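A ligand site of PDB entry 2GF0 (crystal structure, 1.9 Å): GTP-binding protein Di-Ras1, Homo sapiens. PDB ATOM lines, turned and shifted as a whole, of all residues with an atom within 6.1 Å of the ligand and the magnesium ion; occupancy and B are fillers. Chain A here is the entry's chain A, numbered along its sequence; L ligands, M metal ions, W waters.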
ATOM      1  N   GLY A  15      24.502 -24.012   9.961  1.00  0.00           N
ATOM      2  CA  GLY A  15      23.496 -23.986   8.922  1.00  0.00           C
ATOM      3  C   GLY A  15      23.667 -25.167   7.952  1.00  0.00           C
ATOM      4  O   GLY A  15      24.744 -25.809   7.815  1.00  0.00           O
ATOM      5  N   ALA A  16      22.595 -25.408   7.217  1.00  0.00           N
ATOM      6  CA  ALA A  16      22.596 -26.497   6.246  1.00  0.00           C
ATOM      7  C   ALA A  16      23.623 -26.269   5.133  1.00  0.00           C
ATOM      8  O   ALA A  16      24.010 -25.134   4.807  1.00  0.00           O
ATOM      9  CB  ALA A  16      21.160 -26.632   5.639  1.00  0.00           C
ATOM     10  N   GLY A  17      24.012 -27.360   4.494  1.00  0.00           N
ATOM     11  CA  GLY A  17      24.864 -27.294   3.324  1.00  0.00           C
ATOM     12  C   GLY A  17      24.261 -26.378   2.284  1.00  0.00           C
ATOM     13  O   GLY A  17      23.059 -26.465   1.970  1.00  0.00           O
ATOM     14  N   GLY A  18      25.090 -25.493   1.745  1.00  0.00           N
ATOM     15  CA  GLY A  18      24.723 -24.697   0.577  1.00  0.00           C
ATOM     16  C   GLY A  18      24.066 -23.367   0.876  1.00  0.00           C
ATOM     17  O   GLY A  18      23.686 -22.660  -0.066  1.00  0.00           O
ATOM     18  N   VAL A  19      23.907 -23.021   2.142  1.00  0.00           N
ATOM     19  CA  VAL A  19      23.243 -21.748   2.505  1.00  0.00           C
ATOM     20  C   VAL A  19      24.150 -20.511   2.350  1.00  0.00           C
ATOM     21  O   VAL A  19      23.654 -19.401   2.194  1.00  0.00           O
ATOM     22  CB  VAL A  19      22.604 -21.795   3.907  1.00  0.00           C
ATOM     23  CG1 VAL A  19      21.555 -22.916   3.963  1.00  0.00           C
ATOM     24  CG2 VAL A  19      23.658 -21.984   5.040  1.00  0.00           C
ATOM     25  N   GLY A  20      25.464 -20.722   2.327  1.00  0.00           N
ATOM     26  CA  GLY A  20      26.436 -19.636   2.182  1.00  0.00           C
ATOM     27  C   GLY A  20      27.230 -19.353   3.459  1.00  0.00           C
ATOM     28  O   GLY A  20      27.738 -18.232   3.630  1.00  0.00           O
ATOM     29  N   LYS A  21      27.401 -20.348   4.332  1.00  0.00           N
ATOM     30  CA  LYS A  21      28.226 -20.170   5.543  1.00  0.00           C
ATOM     31  C   LYS A  21      29.639 -19.785   5.164  1.00  0.00           C
ATOM     32  O   LYS A  21      30.185 -18.784   5.667  1.00  0.00           O
ATOM     33  CB  LYS A  21      28.275 -21.442   6.393  1.00  0.00           C
ATOM     34  CG  LYS A  21      26.943 -21.903   7.004  1.00  0.00           C
ATOM     35  CD  LYS A  21      27.129 -23.162   7.851  1.00  0.00           C
ATOM     36  CE  LYS A  21      27.588 -24.414   7.090  1.00  0.00           C
ATOM     37  NZ  LYS A  21      26.762 -24.747   5.862  1.00  0.00           N
ATOM     38  N   SER A  22      30.252 -20.560   4.274  1.00  0.00           N
ATOM     39  CA  SER A  22      31.644 -20.300   3.887  1.00  0.00           C
ATOM     40  C   SER A  22      31.750 -18.976   3.141  1.00  0.00           C
ATOM     41  O   SER A  22      32.689 -18.207   3.341  1.00  0.00           O
ATOM     42  CB  SER A  22      32.239 -21.439   3.032  1.00  0.00           C
ATOM     43  OG  SER A  22      32.165 -22.690   3.708  1.00  0.00           O
ATOM     44  N   SER A  23      30.785 -18.676   2.275  1.00  0.00           N
ATOM     45  CA  SER A  23      30.833 -17.432   1.532  1.00  0.00           C
ATOM     46  C   SER A  23      30.722 -16.224   2.460  1.00  0.00           C
ATOM     47  O   SER A  23      31.381 -15.215   2.230  1.00  0.00           O
ATOM     48  CB  SER A  23      29.717 -17.396   0.460  1.00  0.00           C
ATOM     49  OG  SER A  23      29.891 -18.400  -0.540  1.00  0.00           O
ATOM     50  N   LEU A  24      29.871 -16.294   3.487  1.00  0.00           N
ATOM     51  CA  LEU A  24      29.747 -15.207   4.487  1.00  0.00           C
ATOM     52  C   LEU A  24      31.062 -14.992   5.240  1.00  0.00           C
ATOM     53  O   LEU A  24      31.573 -13.880   5.305  1.00  0.00           O
ATOM     54  CB  LEU A  24      28.647 -15.486   5.478  1.00  0.00           C
ATOM     55  CG  LEU A  24      27.249 -15.166   4.932  1.00  0.00           C
ATOM     56  CD1 LEU A  24      26.239 -15.754   5.807  1.00  0.00           C
ATOM     57  CD2 LEU A  24      27.027 -13.631   4.777  1.00  0.00           C
ATOM     58  N   ARG A  34      33.900 -18.111  -1.871  1.00  0.00           N
ATOM     59  CA  ARG A  34      34.119 -19.541  -1.664  1.00  0.00           C
ATOM     60  C   ARG A  34      34.354 -20.260  -2.999  1.00  0.00           C
ATOM     61  O   ARG A  34      33.463 -20.326  -3.852  1.00  0.00           O
ATOM     62  CB  ARG A  34      32.932 -20.175  -0.931  1.00  0.00           C
ATOM     63  CG  ARG A  34      33.037 -21.705  -0.732  1.00  0.00           C
ATOM     64  CD  ARG A  34      34.368 -22.146  -0.110  1.00  0.00           C
ATOM     65  NE  ARG A  34      34.289 -23.379   0.691  1.00  0.00           N
ATOM     66  CZ  ARG A  34      34.373 -24.635   0.219  1.00  0.00           C
ATOM     67  NH1 ARG A  34      34.304 -25.654   1.067  1.00  0.00           N
ATOM     68  NH2 ARG A  34      34.540 -24.886  -1.080  1.00  0.00           N
ATOM     69  N   THR A  36      34.359 -23.238  -5.247  1.00  0.00           N
ATOM     70  CA  THR A  36      33.546 -24.447  -5.165  1.00  0.00           C
ATOM     71  C   THR A  36      34.392 -25.731  -5.051  1.00  0.00           C
ATOM     72  O   THR A  36      33.984 -26.694  -4.391  1.00  0.00           O
ATOM     73  CB  THR A  36      32.523 -24.556  -6.341  1.00  0.00           C
ATOM     74  OG1 THR A  36      31.641 -25.658  -6.090  1.00  0.00           O
ATOM     75  CG2 THR A  36      33.213 -24.759  -7.686  1.00  0.00           C
ATOM     76  N   THR A  40      35.627 -29.492   1.335  1.00  0.00           N
ATOM     77  CA  THR A  40      34.685 -29.097   2.363  1.00  0.00           C
ATOM     78  C   THR A  40      35.130 -29.687   3.715  1.00  0.00           C
ATOM     79  O   THR A  40      34.975 -30.874   3.959  1.00  0.00           O
ATOM     80  CB  THR A  40      33.242 -29.551   1.994  1.00  0.00           C
ATOM     81  OG1 THR A  40      32.868 -28.929   0.749  1.00  0.00           O
ATOM     82  CG2 THR A  40      32.227 -29.164   3.075  1.00  0.00           C
ATOM     83  N   ASP A  62      33.904 -21.917  10.604  1.00  0.00           N
ATOM     84  CA  ASP A  62      33.042 -22.231   9.471  1.00  0.00           C
ATOM     85  C   ASP A  62      32.789 -23.741   9.495  1.00  0.00           C
ATOM     86  O   ASP A  62      33.644 -24.523   9.063  1.00  0.00           O
ATOM     87  CB  ASP A  62      33.782 -21.819   8.171  1.00  0.00           C
ATOM     88  CG  ASP A  62      32.971 -22.077   6.916  1.00  0.00           C
ATOM     89  OD1 ASP A  62      31.735 -22.234   7.059  1.00  0.00           O
ATOM     90  OD2 ASP A  62      33.563 -22.124   5.806  1.00  0.00           O
ATOM     91  N   THR A  63      31.647 -24.160  10.040  1.00  0.00           N
ATOM     92  CA  THR A  63      31.337 -25.579  10.162  1.00  0.00           C
ATOM     93  C   THR A  63      30.930 -26.217   8.829  1.00  0.00           C
ATOM     94  O   THR A  63      30.647 -25.517   7.853  1.00  0.00           O
ATOM     95  CB  THR A  63      30.195 -25.857  11.187  1.00  0.00           C
ATOM     96  OG1 THR A  63      28.953 -25.318  10.719  1.00  0.00           O
ATOM     97  CG2 THR A  63      30.539 -25.264  12.571  1.00  0.00           C
ATOM     98  N   THR A  64      30.889 -27.561   8.795  1.00  0.00           N
ATOM     99  CA  THR A  64      30.425 -28.267   7.581  1.00  0.00           C
ATOM    100  C   THR A  64      28.948 -28.696   7.675  1.00  0.00           C
ATOM    101  O   THR A  64      28.505 -29.623   6.990  1.00  0.00           O
ATOM    102  CB  THR A  64      31.302 -29.459   7.303  1.00  0.00           C
ATOM    103  OG1 THR A  64      31.244 -30.361   8.408  1.00  0.00           O
ATOM    104  CG2 THR A  64      32.742 -29.001   7.143  1.00  0.00           C
ATOM    105  N   ASN A 122      20.550 -15.608   4.437  1.00  0.00           N
ATOM    106  CA  ASN A 122      21.503 -15.303   3.388  1.00  0.00           C
ATOM    107  C   ASN A 122      20.874 -15.506   2.004  1.00  0.00           C
ATOM    108  O   ASN A 122      19.787 -16.094   1.873  1.00  0.00           O
ATOM    109  CB  ASN A 122      22.755 -16.194   3.499  1.00  0.00           C
ATOM    110  CG  ASN A 122      23.886 -15.727   2.578  1.00  0.00           C
ATOM    111  OD1 ASN A 122      24.231 -14.523   2.531  1.00  0.00           O
ATOM    112  ND2 ASN A 122      24.504 -16.676   1.858  1.00  0.00           N
ATOM    113  N   LYS A 123      21.568 -14.967   1.010  1.00  0.00           N
ATOM    114  CA  LYS A 123      21.186 -14.995  -0.406  1.00  0.00           C
ATOM    115  C   LYS A 123      20.012 -14.067  -0.669  1.00  0.00           C
ATOM    116  O   LYS A 123      19.188 -14.329  -1.531  1.00  0.00           O
ATOM    117  CB  LYS A 123      20.846 -16.417  -0.881  1.00  0.00           C
ATOM    118  CG  LYS A 123      21.995 -17.416  -0.743  1.00  0.00           C
ATOM    119  CD  LYS A 123      21.748 -18.698  -1.517  1.00  0.00           C
ATOM    120  CE  LYS A 123      22.779 -19.792  -1.220  1.00  0.00           C
ATOM    121  NZ  LYS A 123      22.587 -20.956  -2.193  1.00  0.00           N
ATOM    122  N   CYS A 124      19.972 -12.953   0.048  1.00  0.00           N
ATOM    123  CA  CYS A 124      18.862 -12.024  -0.103  1.00  0.00           C
ATOM    124  C   CYS A 124      18.940 -11.191  -1.429  1.00  0.00           C
ATOM    125  O   CYS A 124      18.058 -10.367  -1.746  1.00  0.00           O
ATOM    126  CB  CYS A 124      18.733 -11.176   1.158  1.00  0.00           C
ATOM    127  SG  CYS A 124      19.942  -9.834   1.250  1.00  0.00           S
ATOM    128  N   ASP A 125      19.974 -11.454  -2.236  1.00  0.00           N
ATOM    129  CA  ASP A 125      19.990 -11.007  -3.628  1.00  0.00           C
ATOM    130  C   ASP A 125      19.031 -11.786  -4.547  1.00  0.00           C
ATOM    131  O   ASP A 125      18.731 -11.339  -5.646  1.00  0.00           O
ATOM    132  CB  ASP A 125      21.391 -11.094  -4.229  1.00  0.00           C
ATOM    133  CG  ASP A 125      21.958 -12.449  -4.112  1.00  0.00           C
ATOM    134  OD1 ASP A 125      22.402 -12.791  -2.987  1.00  0.00           O
ATOM    135  OD2 ASP A 125      21.914 -13.183  -5.130  1.00  0.00           O
ATOM    136  N   GLU A 126      18.570 -12.922  -4.086  1.00  0.00           N
ATOM    137  CA  GLU A 126      17.673 -13.773  -4.862  1.00  0.00           C
ATOM    138  C   GLU A 126      16.239 -13.287  -4.800  1.00  0.00           C
ATOM    139  O   GLU A 126      15.767 -12.788  -3.767  1.00  0.00           O
ATOM    140  CB  GLU A 126      17.778 -15.204  -4.356  1.00  0.00           C
ATOM    141  CG  GLU A 126      19.148 -15.833  -4.587  1.00  0.00           C
ATOM    142  CD  GLU A 126      19.325 -16.377  -5.992  1.00  0.00           C
ATOM    143  OE1 GLU A 126      18.409 -16.218  -6.810  1.00  0.00           O
ATOM    144  OE2 GLU A 126      20.380 -16.968  -6.260  1.00  0.00           O
ATOM    145  N   THR A 150      21.308 -11.106   4.665  1.00  0.00           N
ATOM    146  CA  THR A 150      22.584 -10.866   4.070  1.00  0.00           C
ATOM    147  C   THR A 150      22.623 -11.377   2.624  1.00  0.00           C
ATOM    148  O   THR A 150      21.831 -12.231   2.229  1.00  0.00           O
ATOM    149  CB  THR A 150      23.720 -11.579   4.859  1.00  0.00           C
ATOM    150  OG1 THR A 150      23.530 -12.990   4.784  1.00  0.00           O
ATOM    151  CG2 THR A 150      23.774 -11.126   6.307  1.00  0.00           C
ATOM    152  N   SER A 151      23.550 -10.816   1.851  1.00  0.00           N
ATOM    153  CA  SER A 151      23.997 -11.380   0.593  1.00  0.00           C
ATOM    154  C   SER A 151      25.522 -11.412   0.650  1.00  0.00           C
ATOM    155  O   SER A 151      26.146 -10.391   0.433  1.00  0.00           O
ATOM    156  CB  SER A 151      23.576 -10.554  -0.596  1.00  0.00           C
ATOM    157  OG  SER A 151      24.097 -11.074  -1.813  1.00  0.00           O
ATOM    158  N   ALA A 152      26.112 -12.577   0.903  1.00  0.00           N
ATOM    159  CA  ALA A 152      27.564 -12.727   0.772  1.00  0.00           C
ATOM    160  C   ALA A 152      28.075 -12.287  -0.604  1.00  0.00           C
ATOM    161  O   ALA A 152      29.124 -11.647  -0.716  1.00  0.00           O
ATOM    162  CB  ALA A 152      27.998 -14.204   1.058  1.00  0.00           C
ATOM    163  N   LYS A 153      27.319 -12.622  -1.638  1.00  0.00           N
ATOM    164  CA  LYS A 153      27.646 -12.325  -2.990  1.00  0.00           C
ATOM    165  C   LYS A 153      27.845 -10.827  -3.211  1.00  0.00           C
ATOM    166  O   LYS A 153      28.762 -10.402  -3.920  1.00  0.00           O
ATOM    167  CB  LYS A 153      26.521 -12.830  -3.907  1.00  0.00           C
ATOM    168  CG  LYS A 153      26.653 -12.441  -5.357  1.00  0.00           C
ATOM    169  CD  LYS A 153      25.562 -13.093  -6.264  1.00  0.00           C
ATOM    170  CE  LYS A 153      25.997 -14.452  -6.750  1.00  0.00           C
ATOM    171  NZ  LYS A 153      27.025 -14.303  -7.818  1.00  0.00           N
ATOM    172  N   MET A 154      26.954 -10.030  -2.646  1.00  0.00           N
ATOM    173  CA  MET A 154      26.942  -8.610  -2.858  1.00  0.00           C
ATOM    174  C   MET A 154      27.646  -7.824  -1.728  1.00  0.00           C
ATOM    175  O   MET A 154      27.690  -6.614  -1.781  1.00  0.00           O
ATOM    176  CB  MET A 154      25.489  -8.147  -2.981  1.00  0.00           C
ATOM    177  CG  MET A 154      24.743  -8.750  -4.205  1.00  0.00           C
ATOM    178  SD  MET A 154      25.607  -8.417  -5.737  1.00  0.00           S
ATOM    179  CE  MET A 154      25.427  -6.628  -5.915  1.00  0.00           C
HETATM  180  P1  LIG L   1      28.000 -23.464   2.671  1.00  0.00           P
HETATM  181  O1  LIG L   1      26.853 -23.068   3.599  1.00  0.00           O
HETATM  182  O2  LIG L   1      27.799 -24.862   2.128  1.00  0.00           O
HETATM  183  O3  LIG L   1      29.388 -23.232   3.212  1.00  0.00           O
HETATM  184  O4  LIG L   1      27.682 -22.486   1.412  1.00  0.00           O
HETATM  185  P2  LIG L   1      28.724 -21.914   0.335  1.00  0.00           P
HETATM  186  O5  LIG L   1      29.700 -22.983  -0.119  1.00  0.00           O
HETATM  187  O6  LIG L   1      29.397 -20.689   0.894  1.00  0.00           O
HETATM  188  O7  LIG L   1      27.778 -21.405  -0.848  1.00  0.00           O
HETATM  189  C1  LIG L   1      26.970 -22.378  -1.483  1.00  0.00           C
HETATM  190  C2  LIG L   1      26.523 -21.858  -2.839  1.00  0.00           C
HETATM  191  O8  LIG L   1      25.672 -20.733  -2.642  1.00  0.00           O
HETATM  192  C3  LIG L   1      27.696 -21.425  -3.706  1.00  0.00           C
HETATM  193  O9  LIG L   1      27.339 -21.643  -5.065  1.00  0.00           O
HETATM  194  C4  LIG L   1      27.757 -19.945  -3.464  1.00  0.00           C
HETATM  195  O10 LIG L   1      28.335 -19.265  -4.569  1.00  0.00           O
HETATM  196  C5  LIG L   1      26.265 -19.631  -3.287  1.00  0.00           C
HETATM  197  N1  LIG L   1      26.076 -18.434  -2.471  1.00  0.00           N
HETATM  198  C6  LIG L   1      26.702 -18.162  -1.308  1.00  0.00           C
HETATM  199  N2  LIG L   1      26.312 -16.977  -0.817  1.00  0.00           N
HETATM  200  C7  LIG L   1      25.417 -16.466  -1.714  1.00  0.00           C
HETATM  201  C8  LIG L   1      24.590 -15.244  -1.811  1.00  0.00           C
HETATM  202  O11 LIG L   1      24.607 -14.342  -0.959  1.00  0.00           O
HETATM  203  N3  LIG L   1      23.800 -15.124  -2.892  1.00  0.00           N
HETATM  204  C9  LIG L   1      23.711 -16.058  -3.849  1.00  0.00           C
HETATM  205  N4  LIG L   1      22.867 -15.816  -4.883  1.00  0.00           N
HETATM  206  N5  LIG L   1      24.417 -17.207  -3.843  1.00  0.00           N
HETATM  207  C10 LIG L   1      25.271 -17.442  -2.792  1.00  0.00           C
HETATM  208 MG    MG M   1      31.054 -24.337   3.398  1.00  0.00          MG
HETATM  209  O   HOH W   1      30.782 -24.100   5.489  1.00  0.00           O
HETATM  210  O   HOH W   2      30.016 -25.985   3.195  1.00  0.00           O
HETATM  211  O   HOH W   3      23.014 -19.773  -4.737  1.00  0.00           O
HETATM  212  O   HOH W   4      29.348 -20.598  -7.031  1.00  0.00           O
HETATM  213  O   HOH W   5      28.923 -15.920  -4.042  1.00  0.00           O
HETATM  214  O   HOH W   6      32.792 -25.486   3.697  1.00  0.00           O
HETATM  215  O   HOH W   7      31.240 -24.343   1.383  1.00  0.00           O
HETATM  216  O   HOH W   8      27.928 -26.322   0.014  1.00  0.00           O
HETATM  217  O   HOH W   9      30.502 -23.808  -2.730  1.00  0.00           O
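O of Ala 16 touches O1 of the ligand, 3.7 Å away. Gly 17 touches the ligand (C to O2, 3.9 Å). Arg 34 touches the ligand. Hydrophobic or aromatic side chains within 4 Å of the ligand: Val 19 and Ala 152. 16 residues have an atom within 4 Å of the ligand: Ala 16, Gly 17, Gly 18, Val 19, Gly 20, Lys 21, Ser 22, Ser 23, Arg 34, Asn 122, Lys 123, Asp 125, Glu 126, Ser 151, Ala 152 and Lys 153. The nearest printed residue that does not touch the ligand is Asp 62 (4.6 Å).
Water W7 lies within hydrogen-bond range of O5 of the ligand (2.5 Å) and NE of Arg 34 (3.3 Å). Water W1 bridges the side-chain carboxylate of Asp 62 (2.6 Å) and the backbone carbonyl oxygen of Thr 63 (2.8 Å). Water W8 bridges O2 of the ligand (2.6 Å) and N of Gly 18 (3.4 Å). Water W3 bridges the side-chain amino group of Lys 123 (2.8 Å) and a nitrogen (N5) of the ligand (3.1 Å).
One residue has an atom within 4 Å of the magnesium ion: Ser 22.
The backbone NH (N) of Ser 22 lies within hydrogen-bond range of an oxygen (O6) of the ligand. The side-chain carboxylate of Asp 125 sits at hydrogen-bond distance from a nitrogen (N3) of the ligand, 2.7 Å away. An oxygen (O6) of the ligand lies within hydrogen-bond range of the backbone NH of Ser 23 (2.8 Å). O6 of the ligand sits at hydrogen-bond distance from OG of Ser 23. The backbone NH of Gly 18 sits at hydrogen-bond distance from an oxygen (O2) of the ligand (2.8 Å). N of Lys 21 sits at hydrogen-bond distance from O1 of the ligand. The side-chain amino group (NZ) of Lys 21 lies within salt-bridge range of an oxygen (O1) of the ligand (2.8 Å). O11 of the ligand is in hydrogen-bond range of N of Ala 152, 3.0 Å away. N of Gly 20 is in hydrogen-bond range of O4 of the ligand (3.0 Å). N4 of the ligand sits at hydrogen-bond distance from OE2 of Glu 126, 3.1 Å away. NZ of Lys 123 lies within hydrogen-bond range of O8 of the ligand. A nitrogen (N2) of the ligand is in hydrogen-bond range of the side-chain amide nitrogen (ND2) of Asn 122. O11 of the ligand sits at hydrogen-bond distance from N of Lys 153, at 3.3 Å. N of Val 19 is in hydrogen-bond range of O1 of the ligand, 3.3 Å away. OG of Ser 151 sits close to O11 of the ligand, 3.4 Å away.
The magnesium ion is bound by water W2. O3 of the ligand is bound to the magnesium ion (2.0 Å). The side-chain hydroxyl (OG) of Ser 22 binds the magnesium ion, 2.0 Å away. The magnesium ion is bound by water W7, at 2.0 Å. Water W6 is bound to the magnesium ion. The magnesium ion is bound by water W1. The magnesium ion has six donor atoms within binding distance.
The side-chain hydroxyl (OG) of Ser 22 lies close to the side-chain carboxylate (OD2) of Asp 62 (2.6 Å). The backbone carbonyl oxygen (O) of Gly 18 sits at hydrogen-bond distance from the side-chain amino group (NZ) of Lys 123, 2.9 Å away. OD1 of Asn 122 sits at hydrogen-bond distance from N of Ala 152. The backbone NH (N) of Lys 123 lies within hydrogen-bond range of the backbone carbonyl oxygen (O) of Thr 150 (3.0 Å). The backbone carbonyl oxygen (O) of Val 19 lies within hydrogen-bond range of the side-chain amide nitrogen (ND2) of Asn 122. The side-chain amide oxygen (OD1) of Asn 122 sits at hydrogen-bond distance from the side-chain hydroxyl (OG1) of Thr 150 (2.8 Å). The backbone NH (N) of Ser 151 sits at hydrogen-bond distance from the side-chain sulfur (SG) of Cys 124 (3.8 Å). The side-chain hydroxyl of Ser 151 is in hydrogen-bond range of the backbone NH of Met 154.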
